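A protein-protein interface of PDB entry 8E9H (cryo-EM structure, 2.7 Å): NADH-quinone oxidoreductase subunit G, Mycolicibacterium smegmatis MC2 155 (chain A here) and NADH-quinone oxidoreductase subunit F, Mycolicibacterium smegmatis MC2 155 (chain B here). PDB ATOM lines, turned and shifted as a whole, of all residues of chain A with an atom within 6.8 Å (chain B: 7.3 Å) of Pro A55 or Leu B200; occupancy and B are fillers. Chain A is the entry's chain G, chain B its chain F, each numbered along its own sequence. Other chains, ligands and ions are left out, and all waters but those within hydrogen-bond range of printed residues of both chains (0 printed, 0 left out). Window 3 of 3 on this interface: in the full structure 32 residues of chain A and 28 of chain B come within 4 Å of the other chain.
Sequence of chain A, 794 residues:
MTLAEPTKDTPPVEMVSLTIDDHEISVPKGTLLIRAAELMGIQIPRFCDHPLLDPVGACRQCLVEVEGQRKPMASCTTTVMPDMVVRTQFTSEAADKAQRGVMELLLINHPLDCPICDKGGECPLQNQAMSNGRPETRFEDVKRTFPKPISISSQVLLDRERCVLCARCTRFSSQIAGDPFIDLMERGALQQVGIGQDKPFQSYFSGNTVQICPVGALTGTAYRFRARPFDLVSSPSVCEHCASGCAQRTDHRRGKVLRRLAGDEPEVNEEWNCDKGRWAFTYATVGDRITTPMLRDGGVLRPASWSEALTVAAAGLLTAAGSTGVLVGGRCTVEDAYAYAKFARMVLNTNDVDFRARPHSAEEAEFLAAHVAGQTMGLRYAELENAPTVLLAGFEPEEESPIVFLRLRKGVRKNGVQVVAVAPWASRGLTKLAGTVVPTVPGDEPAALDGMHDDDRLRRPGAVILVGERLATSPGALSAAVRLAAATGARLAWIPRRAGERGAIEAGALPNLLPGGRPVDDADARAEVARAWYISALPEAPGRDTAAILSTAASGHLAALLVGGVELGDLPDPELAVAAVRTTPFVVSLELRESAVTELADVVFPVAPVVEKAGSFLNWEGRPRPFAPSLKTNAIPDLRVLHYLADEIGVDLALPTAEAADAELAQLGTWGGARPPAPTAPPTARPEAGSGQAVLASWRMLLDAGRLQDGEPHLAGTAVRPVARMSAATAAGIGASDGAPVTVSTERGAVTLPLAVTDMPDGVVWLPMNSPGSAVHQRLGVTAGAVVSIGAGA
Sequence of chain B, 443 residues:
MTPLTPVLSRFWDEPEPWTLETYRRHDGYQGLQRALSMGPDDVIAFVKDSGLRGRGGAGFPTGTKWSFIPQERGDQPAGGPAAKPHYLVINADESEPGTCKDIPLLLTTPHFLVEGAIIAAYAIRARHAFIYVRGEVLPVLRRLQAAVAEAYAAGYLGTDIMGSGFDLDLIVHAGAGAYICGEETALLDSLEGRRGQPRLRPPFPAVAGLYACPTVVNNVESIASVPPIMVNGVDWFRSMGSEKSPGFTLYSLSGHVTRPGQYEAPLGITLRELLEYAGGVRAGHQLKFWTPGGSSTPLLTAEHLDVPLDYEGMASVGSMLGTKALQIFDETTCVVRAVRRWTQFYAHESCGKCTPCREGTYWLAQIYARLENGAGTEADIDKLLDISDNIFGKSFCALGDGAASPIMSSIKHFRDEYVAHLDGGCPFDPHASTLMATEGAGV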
ATOM      1  N   LEU A  32      30.755  -6.872  -9.763  1.00  0.00           N
ATOM      2  CA  LEU A  32      30.711  -5.652 -10.550  1.00  0.00           C
ATOM      3  C   LEU A  32      30.938  -4.438  -9.660  1.00  0.00           C
ATOM      4  O   LEU A  32      30.538  -4.412  -8.494  1.00  0.00           O
ATOM      5  CB  LEU A  32      29.371  -5.527 -11.268  1.00  0.00           C
ATOM      6  CG  LEU A  32      29.111  -6.588 -12.332  1.00  0.00           C
ATOM      7  CD1 LEU A  32      27.645  -6.601 -12.710  1.00  0.00           C
ATOM      8  CD2 LEU A  32      29.974  -6.340 -13.549  1.00  0.00           C
ATOM      9  N   CYS A  48      20.117   0.876 -16.666  1.00  0.00           N
ATOM     10  CA  CYS A  48      20.082  -0.414 -17.340  1.00  0.00           C
ATOM     11  C   CYS A  48      20.627  -1.543 -16.484  1.00  0.00           C
ATOM     12  O   CYS A  48      20.405  -2.710 -16.813  1.00  0.00           O
ATOM     13  CB  CYS A  48      20.859  -0.350 -18.653  1.00  0.00           C
ATOM     14  SG  CYS A  48      22.638  -0.360 -18.471  1.00  0.00           S
ATOM     15  N   ASP A  49      21.329  -1.232 -15.402  1.00  0.00           N
ATOM     16  CA  ASP A  49      21.836  -2.283 -14.537  1.00  0.00           C
ATOM     17  C   ASP A  49      20.698  -2.938 -13.770  1.00  0.00           C
ATOM     18  O   ASP A  49      19.736  -2.278 -13.371  1.00  0.00           O
ATOM     19  CB  ASP A  49      22.854  -1.721 -13.555  1.00  0.00           C
ATOM     20  CG  ASP A  49      23.458  -2.789 -12.683  1.00  0.00           C
ATOM     21  OD1 ASP A  49      23.864  -3.835 -13.228  1.00  0.00           O
ATOM     22  OD2 ASP A  49      23.513  -2.598 -11.452  1.00  0.00           O
ATOM     23  N   HIS A  50      20.812  -4.246 -13.562  1.00  0.00           N
ATOM     24  CA  HIS A  50      19.876  -4.956 -12.733  1.00  0.00           C
ATOM     25  C   HIS A  50      20.654  -6.100 -12.103  1.00  0.00           C
ATOM     26  O   HIS A  50      21.314  -6.852 -12.835  1.00  0.00           O
ATOM     27  CB  HIS A  50      18.686  -5.504 -13.506  1.00  0.00           C
ATOM     28  CG  HIS A  50      17.547  -5.914 -12.632  1.00  0.00           C
ATOM     29  ND1 HIS A  50      17.610  -6.998 -11.786  1.00  0.00           N
ATOM     30  CD2 HIS A  50      16.310  -5.392 -12.483  1.00  0.00           C
ATOM     31  CE1 HIS A  50      16.463  -7.117 -11.143  1.00  0.00           C
ATOM     32  NE2 HIS A  50      15.657  -6.156 -11.549  1.00  0.00           N
ATOM     33  N   LEU A  53      19.798  -9.367 -13.805  1.00  0.00           N
ATOM     34  CA  LEU A  53      19.962  -9.464 -15.246  1.00  0.00           C
ATOM     35  C   LEU A  53      21.436  -9.394 -15.617  1.00  0.00           C
ATOM     36  O   LEU A  53      22.240  -8.742 -14.950  1.00  0.00           O
ATOM     37  CB  LEU A  53      19.202  -8.351 -15.959  1.00  0.00           C
ATOM     38  CG  LEU A  53      17.703  -8.269 -15.702  1.00  0.00           C
ATOM     39  CD1 LEU A  53      17.115  -7.125 -16.487  1.00  0.00           C
ATOM     40  CD2 LEU A  53      17.027  -9.567 -16.070  1.00  0.00           C
ATOM     41  N   ASP A  54      21.784 -10.076 -16.698  1.00  0.00           N
ATOM     42  CA  ASP A  54      23.145 -10.002 -17.195  1.00  0.00           C
ATOM     43  C   ASP A  54      23.449  -8.565 -17.611  1.00  0.00           C
ATOM     44  O   ASP A  54      22.653  -7.945 -18.323  1.00  0.00           O
ATOM     45  CB  ASP A  54      23.339 -10.947 -18.379  1.00  0.00           C
ATOM     46  N   PRO A  55      24.577  -8.002 -17.190  1.00  0.00           N
ATOM     47  CA  PRO A  55      24.837  -6.590 -17.479  1.00  0.00           C
ATOM     48  C   PRO A  55      24.885  -6.323 -18.971  1.00  0.00           C
ATOM     49  O   PRO A  55      25.329  -7.155 -19.763  1.00  0.00           O
ATOM     50  CB  PRO A  55      26.198  -6.340 -16.824  1.00  0.00           C
ATOM     51  CG  PRO A  55      26.835  -7.669 -16.778  1.00  0.00           C
ATOM     52  CD  PRO A  55      25.725  -8.634 -16.522  1.00  0.00           C
ATOM     53  N   VAL A  56      24.409  -5.138 -19.348  1.00  0.00           N
ATOM     54  CA  VAL A  56      24.395  -4.733 -20.750  1.00  0.00           C
ATOM     55  C   VAL A  56      25.133  -3.432 -21.004  1.00  0.00           C
ATOM     56  O   VAL A  56      25.554  -3.183 -22.148  1.00  0.00           O
ATOM     57  CB  VAL A  56      22.943  -4.631 -21.261  1.00  0.00           C
ATOM     58  CG1 VAL A  56      22.235  -3.455 -20.627  1.00  0.00           C
ATOM     59  CG2 VAL A  56      22.923  -4.511 -22.767  1.00  0.00           C
ATOM     60  N   GLY A  57      25.326  -2.570 -20.010  1.00  0.00           N
ATOM     61  CA  GLY A  57      26.072  -1.349 -20.227  1.00  0.00           C
ATOM     62  C   GLY A  57      25.481  -0.435 -21.269  1.00  0.00           C
ATOM     63  O   GLY A  57      26.224   0.171 -22.039  1.00  0.00           O
ATOM     64  N   ALA A  58      24.156  -0.309 -21.312  1.00  0.00           N
ATOM     65  CA  ALA A  58      23.520   0.442 -22.387  1.00  0.00           C
ATOM     66  C   ALA A  58      23.393   1.915 -22.035  1.00  0.00           C
ATOM     67  O   ALA A  58      23.903   2.783 -22.751  1.00  0.00           O
ATOM     68  CB  ALA A  58      22.148  -0.153 -22.693  1.00  0.00           C
ATOM     69  N   CYS A  76      28.496  -0.836 -14.040  1.00  0.00           N
ATOM     70  CA  CYS A  76      27.605  -1.982 -14.134  1.00  0.00           C
ATOM     71  C   CYS A  76      28.163  -3.091 -15.011  1.00  0.00           C
ATOM     72  O   CYS A  76      27.598  -4.186 -15.021  1.00  0.00           O
ATOM     73  CB  CYS A  76      26.241  -1.547 -14.669  1.00  0.00           C
ATOM     74  SG  CYS A  76      26.135  -1.451 -16.458  1.00  0.00           S
ATOM     75  N   THR A  77      29.246  -2.836 -15.741  1.00  0.00           N
ATOM     76  CA  THR A  77      29.876  -3.843 -16.575  1.00  0.00           C
ATOM     77  C   THR A  77      31.315  -4.130 -16.193  1.00  0.00           C
ATOM     78  O   THR A  77      31.944  -4.981 -16.828  1.00  0.00           O
ATOM     79  CB  THR A  77      29.852  -3.415 -18.047  1.00  0.00           C
ATOM     80  OG1 THR A  77      30.803  -2.366 -18.251  1.00  0.00           O
ATOM     81  CG2 THR A  77      28.480  -2.925 -18.435  1.00  0.00           C
ATOM     82  N   THR A  78      31.852  -3.451 -15.188  1.00  0.00           N
ATOM     83  CA  THR A  78      33.256  -3.561 -14.832  1.00  0.00           C
ATOM     84  C   THR A  78      33.407  -4.547 -13.684  1.00  0.00           C
ATOM     85  O   THR A  78      32.850  -4.336 -12.603  1.00  0.00           O
ATOM     86  CB  THR A  78      33.819  -2.198 -14.438  1.00  0.00           C
ATOM     87  OG1 THR A  78      33.600  -1.267 -15.501  1.00  0.00           O
ATOM     88  CG2 THR A  78      35.301  -2.297 -14.149  1.00  0.00           C
ATOM     89  N   ARG A 171      15.508  -7.527 -21.666  1.00  0.00           N
ATOM     90  CA  ARG A 171      16.503  -8.418 -21.088  1.00  0.00           C
ATOM     91  C   ARG A 171      15.858  -9.387 -20.111  1.00  0.00           C
ATOM     92  O   ARG A 171      16.285 -10.539 -20.002  1.00  0.00           O
ATOM     93  CB  ARG A 171      17.597  -7.603 -20.406  1.00  0.00           C
ATOM     94  CG  ARG A 171      18.577  -6.994 -21.378  1.00  0.00           C
ATOM     95  CD  ARG A 171      19.240  -5.762 -20.809  1.00  0.00           C
ATOM     96  NE  ARG A 171      19.924  -6.040 -19.553  1.00  0.00           N
ATOM     97  CZ  ARG A 171      19.973  -5.211 -18.520  1.00  0.00           C
ATOM     98  NH1 ARG A 171      19.413  -4.016 -18.562  1.00  0.00           N
ATOM     99  NH2 ARG A 171      20.607  -5.591 -17.418  1.00  0.00           N
ATOM    100  N   GLN A 175      16.173 -13.309 -20.751  1.00  0.00           N
ATOM    101  CA  GLN A 175      16.985 -14.091 -19.828  1.00  0.00           C
ATOM    102  C   GLN A 175      16.124 -14.781 -18.780  1.00  0.00           C
ATOM    103  O   GLN A 175      16.082 -16.013 -18.705  1.00  0.00           O
ATOM    104  CB  GLN A 175      18.012 -13.178 -19.160  1.00  0.00           C
ATOM    105  CG  GLN A 175      18.610 -13.732 -17.891  1.00  0.00           C
ATOM    106  CD  GLN A 175      19.799 -12.931 -17.424  1.00  0.00           C
ATOM    107  OE1 GLN A 175      20.217 -11.981 -18.083  1.00  0.00           O
ATOM    108  NE2 GLN A 175      20.347 -13.301 -16.275  1.00  0.00           N
ATOM    109  N   THR B 185      31.721  -7.286 -33.189  1.00  0.00           N
ATOM    110  CA  THR B 185      30.690  -7.609 -32.211  1.00  0.00           C
ATOM    111  C   THR B 185      29.340  -7.031 -32.609  1.00  0.00           C
ATOM    112  O   THR B 185      28.314  -7.387 -32.023  1.00  0.00           O
ATOM    113  CB  THR B 185      31.074  -7.091 -30.825  1.00  0.00           C
ATOM    114  OG1 THR B 185      30.957  -5.664 -30.793  1.00  0.00           O
ATOM    115  CG2 THR B 185      32.489  -7.495 -30.465  1.00  0.00           C
ATOM    116  N   ASP B 189      27.075  -9.856 -34.346  1.00  0.00           N
ATOM    117  CA  ASP B 189      25.664  -9.930 -33.985  1.00  0.00           C
ATOM    118  C   ASP B 189      24.785 -10.013 -35.223  1.00  0.00           C
ATOM    119  O   ASP B 189      23.819 -10.783 -35.253  1.00  0.00           O
ATOM    120  CB  ASP B 189      25.279  -8.725 -33.133  1.00  0.00           C
ATOM    121  CG  ASP B 189      25.646  -8.906 -31.677  1.00  0.00           C
ATOM    122  OD1 ASP B 189      26.383  -9.862 -31.364  1.00  0.00           O
ATOM    123  OD2 ASP B 189      25.193  -8.093 -30.845  1.00  0.00           O
ATOM    124  N   GLN B 197      24.058  -4.613 -33.037  1.00  0.00           N
ATOM    125  CA  GLN B 197      24.488  -3.723 -31.972  1.00  0.00           C
ATOM    126  C   GLN B 197      25.769  -4.237 -31.331  1.00  0.00           C
ATOM    127  O   GLN B 197      25.927  -5.446 -31.147  1.00  0.00           O
ATOM    128  CB  GLN B 197      23.405  -3.603 -30.905  1.00  0.00           C
ATOM    129  CG  GLN B 197      22.090  -3.094 -31.436  1.00  0.00           C
ATOM    130  CD  GLN B 197      21.195  -2.572 -30.343  1.00  0.00           C
ATOM    131  OE1 GLN B 197      21.205  -3.080 -29.227  1.00  0.00           O
ATOM    132  NE2 GLN B 197      20.415  -1.550 -30.656  1.00  0.00           N
ATOM    133  N   PRO B 198      26.700  -3.356 -30.968  1.00  0.00           N
ATOM    134  CA  PRO B 198      27.956  -3.824 -30.376  1.00  0.00           C
ATOM    135  C   PRO B 198      27.721  -4.596 -29.091  1.00  0.00           C
ATOM    136  O   PRO B 198      26.772  -4.339 -28.348  1.00  0.00           O
ATOM    137  CB  PRO B 198      28.726  -2.529 -30.113  1.00  0.00           C
ATOM    138  CG  PRO B 198      28.145  -1.553 -31.049  1.00  0.00           C
ATOM    139  CD  PRO B 198      26.703  -1.899 -31.154  1.00  0.00           C
ATOM    140  N   ARG B 199      28.598  -5.557 -28.835  1.00  0.00           N
ATOM    141  CA  ARG B 199      28.522  -6.355 -27.624  1.00  0.00           C
ATOM    142  C   ARG B 199      29.321  -5.710 -26.504  1.00  0.00           C
ATOM    143  O   ARG B 199      30.116  -4.793 -26.712  1.00  0.00           O
ATOM    144  CB  ARG B 199      29.055  -7.764 -27.852  1.00  0.00           C
ATOM    145  CG  ARG B 199      28.290  -8.580 -28.853  1.00  0.00           C
ATOM    146  CD  ARG B 199      29.037  -9.859 -29.137  1.00  0.00           C
ATOM    147  NE  ARG B 199      28.418 -10.636 -30.199  1.00  0.00           N
ATOM    148  CZ  ARG B 199      28.795 -11.858 -30.540  1.00  0.00           C
ATOM    149  NH1 ARG B 199      29.795 -12.470 -29.928  1.00  0.00           N
ATOM    150  NH2 ARG B 199      28.151 -12.485 -31.519  1.00  0.00           N
ATOM    151  N   LEU B 200      29.101  -6.218 -25.301  1.00  0.00           N
ATOM    152  CA  LEU B 200      29.882  -5.804 -24.149  1.00  0.00           C
ATOM    153  C   LEU B 200      31.210  -6.548 -24.139  1.00  0.00           C
ATOM    154  O   LEU B 200      31.245  -7.777 -24.238  1.00  0.00           O
ATOM    155  CB  LEU B 200      29.097  -6.091 -22.875  1.00  0.00           C
ATOM    156  CG  LEU B 200      29.594  -5.505 -21.562  1.00  0.00           C
ATOM    157  CD1 LEU B 200      28.403  -5.333 -20.650  1.00  0.00           C
ATOM    158  CD2 LEU B 200      30.639  -6.395 -20.921  1.00  0.00           C
ATOM    159  N   ARG B 201      32.304  -5.805 -24.024  1.00  0.00           N
ATOM    160  CA  ARG B 201      33.629  -6.396 -23.984  1.00  0.00           C
ATOM    161  C   ARG B 201      34.304  -6.095 -22.651  1.00  0.00           C
ATOM    162  O   ARG B 201      34.288  -4.945 -22.203  1.00  0.00           O
ATOM    163  CB  ARG B 201      34.503  -5.859 -25.118  1.00  0.00           C
ATOM    164  CG  ARG B 201      34.002  -6.215 -26.495  1.00  0.00           C
ATOM    165  CD  ARG B 201      34.948  -5.724 -27.566  1.00  0.00           C
ATOM    166  NE  ARG B 201      34.845  -4.282 -27.739  1.00  0.00           N
ATOM    167  CZ  ARG B 201      34.046  -3.681 -28.610  1.00  0.00           C
ATOM    168  NH1 ARG B 201      33.241  -4.369 -29.403  1.00  0.00           N
ATOM    169  NH2 ARG B 201      34.048  -2.353 -28.681  1.00  0.00           N
ATOM    170  N   PRO B 202      34.910  -7.093 -21.990  1.00  0.00           N
ATOM    171  CA  PRO B 202      35.016  -8.502 -22.375  1.00  0.00           C
ATOM    172  C   PRO B 202      33.693  -9.233 -22.220  1.00  0.00           C
ATOM    173  O   PRO B 202      32.777  -8.687 -21.613  1.00  0.00           O
ATOM    174  CB  PRO B 202      36.058  -9.047 -21.400  1.00  0.00           C
ATOM    175  CG  PRO B 202      35.907  -8.203 -20.206  1.00  0.00           C
ATOM    176  CD  PRO B 202      35.612  -6.831 -20.723  1.00  0.00           C
ATOM    177  N   PRO B 203      33.590 -10.455 -22.759  1.00  0.00           N
ATOM    178  CA  PRO B 203      34.646 -11.174 -23.477  1.00  0.00           C
ATOM    179  C   PRO B 203      34.867 -10.641 -24.883  1.00  0.00           C
ATOM    180  O   PRO B 203      33.933 -10.140 -25.503  1.00  0.00           O
ATOM    181  CB  PRO B 203      34.118 -12.603 -23.513  1.00  0.00           C
ATOM    182  CG  PRO B 203      32.647 -12.439 -23.542  1.00  0.00           C
ATOM    183  CD  PRO B 203      32.353 -11.246 -22.681  1.00  0.00           C
ATOM    184  N   PHE B 204      36.092 -10.748 -25.374  1.00  0.00           N
ATOM    185  CA  PHE B 204      36.428 -10.228 -26.683  1.00  0.00           C
ATOM    186  C   PHE B 204      36.141 -11.257 -27.766  1.00  0.00           C
ATOM    187  O   PHE B 204      36.007 -12.450 -27.485  1.00  0.00           O
ATOM    188  CB  PHE B 204      37.895  -9.824 -26.717  1.00  0.00           C
ATOM    189  CG  PHE B 204      38.193  -8.593 -25.925  1.00  0.00           C
ATOM    190  CD1 PHE B 204      38.141  -7.346 -26.517  1.00  0.00           C
ATOM    191  CD2 PHE B 204      38.510  -8.679 -24.583  1.00  0.00           C
ATOM    192  CE1 PHE B 204      38.409  -6.209 -25.789  1.00  0.00           C
ATOM    193  CE2 PHE B 204      38.779  -7.545 -23.850  1.00  0.00           C
ATOM    194  CZ  PHE B 204      38.728  -6.309 -24.453  1.00  0.00           C
ATOM    195  N   LYS B 353      21.524   1.762 -28.878  1.00  0.00           N
ATOM    196  CA  LYS B 353      21.791   1.138 -27.589  1.00  0.00           C
ATOM    197  C   LYS B 353      22.202   2.175 -26.553  1.00  0.00           C
ATOM    198  O   LYS B 353      21.686   2.188 -25.432  1.00  0.00           O
ATOM    199  CB  LYS B 353      22.875   0.072 -27.745  1.00  0.00           C
ATOM    200  CG  LYS B 353      23.501  -0.368 -26.438  1.00  0.00           C
ATOM    201  CD  LYS B 353      24.504  -1.486 -26.631  1.00  0.00           C
ATOM    202  CE  LYS B 353      23.844  -2.842 -26.645  1.00  0.00           C
ATOM    203  NZ  LYS B 353      24.845  -3.924 -26.477  1.00  0.00           N
ATOM    204  N   PHE B 396      28.943   3.613 -25.775  1.00  0.00           N
ATOM    205  CA  PHE B 396      29.268   2.200 -25.621  1.00  0.00           C
ATOM    206  C   PHE B 396      30.307   1.744 -26.632  1.00  0.00           C
ATOM    207  O   PHE B 396      31.218   0.987 -26.280  1.00  0.00           O
ATOM    208  CB  PHE B 396      27.995   1.372 -25.757  1.00  0.00           C
ATOM    209  CG  PHE B 396      28.180  -0.084 -25.507  1.00  0.00           C
ATOM    210  CD1 PHE B 396      28.101  -0.593 -24.232  1.00  0.00           C
ATOM    211  CD2 PHE B 396      28.398  -0.949 -26.554  1.00  0.00           C
ATOM    212  CE1 PHE B 396      28.255  -1.934 -24.006  1.00  0.00           C
ATOM    213  CE2 PHE B 396      28.552  -2.289 -26.333  1.00  0.00           C
ATOM    214  CZ  PHE B 396      28.480  -2.782 -25.059  1.00  0.00           C
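Pro A55 touches Leu B200 (O to CD1, 3.7 Å).
Leu B200 touches Val A56.
O of Val A56 touches CE1 of Phe B396 (3.5 Å).
CD1 of Phe B396 touches O of Gly A57, at 3.0 Å.
Lys B353 touches Ala A58.
CG2 of Thr A77 touches CD1 of Leu B200 (3.3 Å).
Of the 12 printed residues of chain B, 3 touch a printed residue of chain A.
Hydrophobic or aromatic side chains of chain B that line the printed part of chain A: Leu B200 and Phe B396.
Hydrophobic or aromatic side chains of chain A within 4 Å of the printed part of chain B: Ala A58.
Among the printed residues, no Asp or Glu carboxylate lies within 4 Å of a Lys or Arg side-chain nitrogen of the other chain.
Of chain B, only Leu B200 comes within 4 Å of Pro A55.
Of chain A, only Pro A55 (3.7 Å), Val A56 (3.8 Å) and Thr A77 (3.3 Å) come within 4 Å of Leu B200.
Of the printed residues of chain B, Gly A57 touches Phe B396.
Printed residues of chain B within 4 Å of Val A56: Leu B200 and Phe B396.
Of the printed residues of chain A, Phe B396 touches Val A56 and Gly A57.
Thr B185 touches none of the printed residues of chain A.
The nearest printed residue of chain A that does not touch Phe B396 is Ala A58 (4.9 Å).
The backbone carbonyl oxygen of Pro B198 is in hydrogen-bond range of the side-chain amino group of Lys B353 (2.7 Å).
SG of Cys A48 sits close to N of Ala A58 (3.2 Å).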
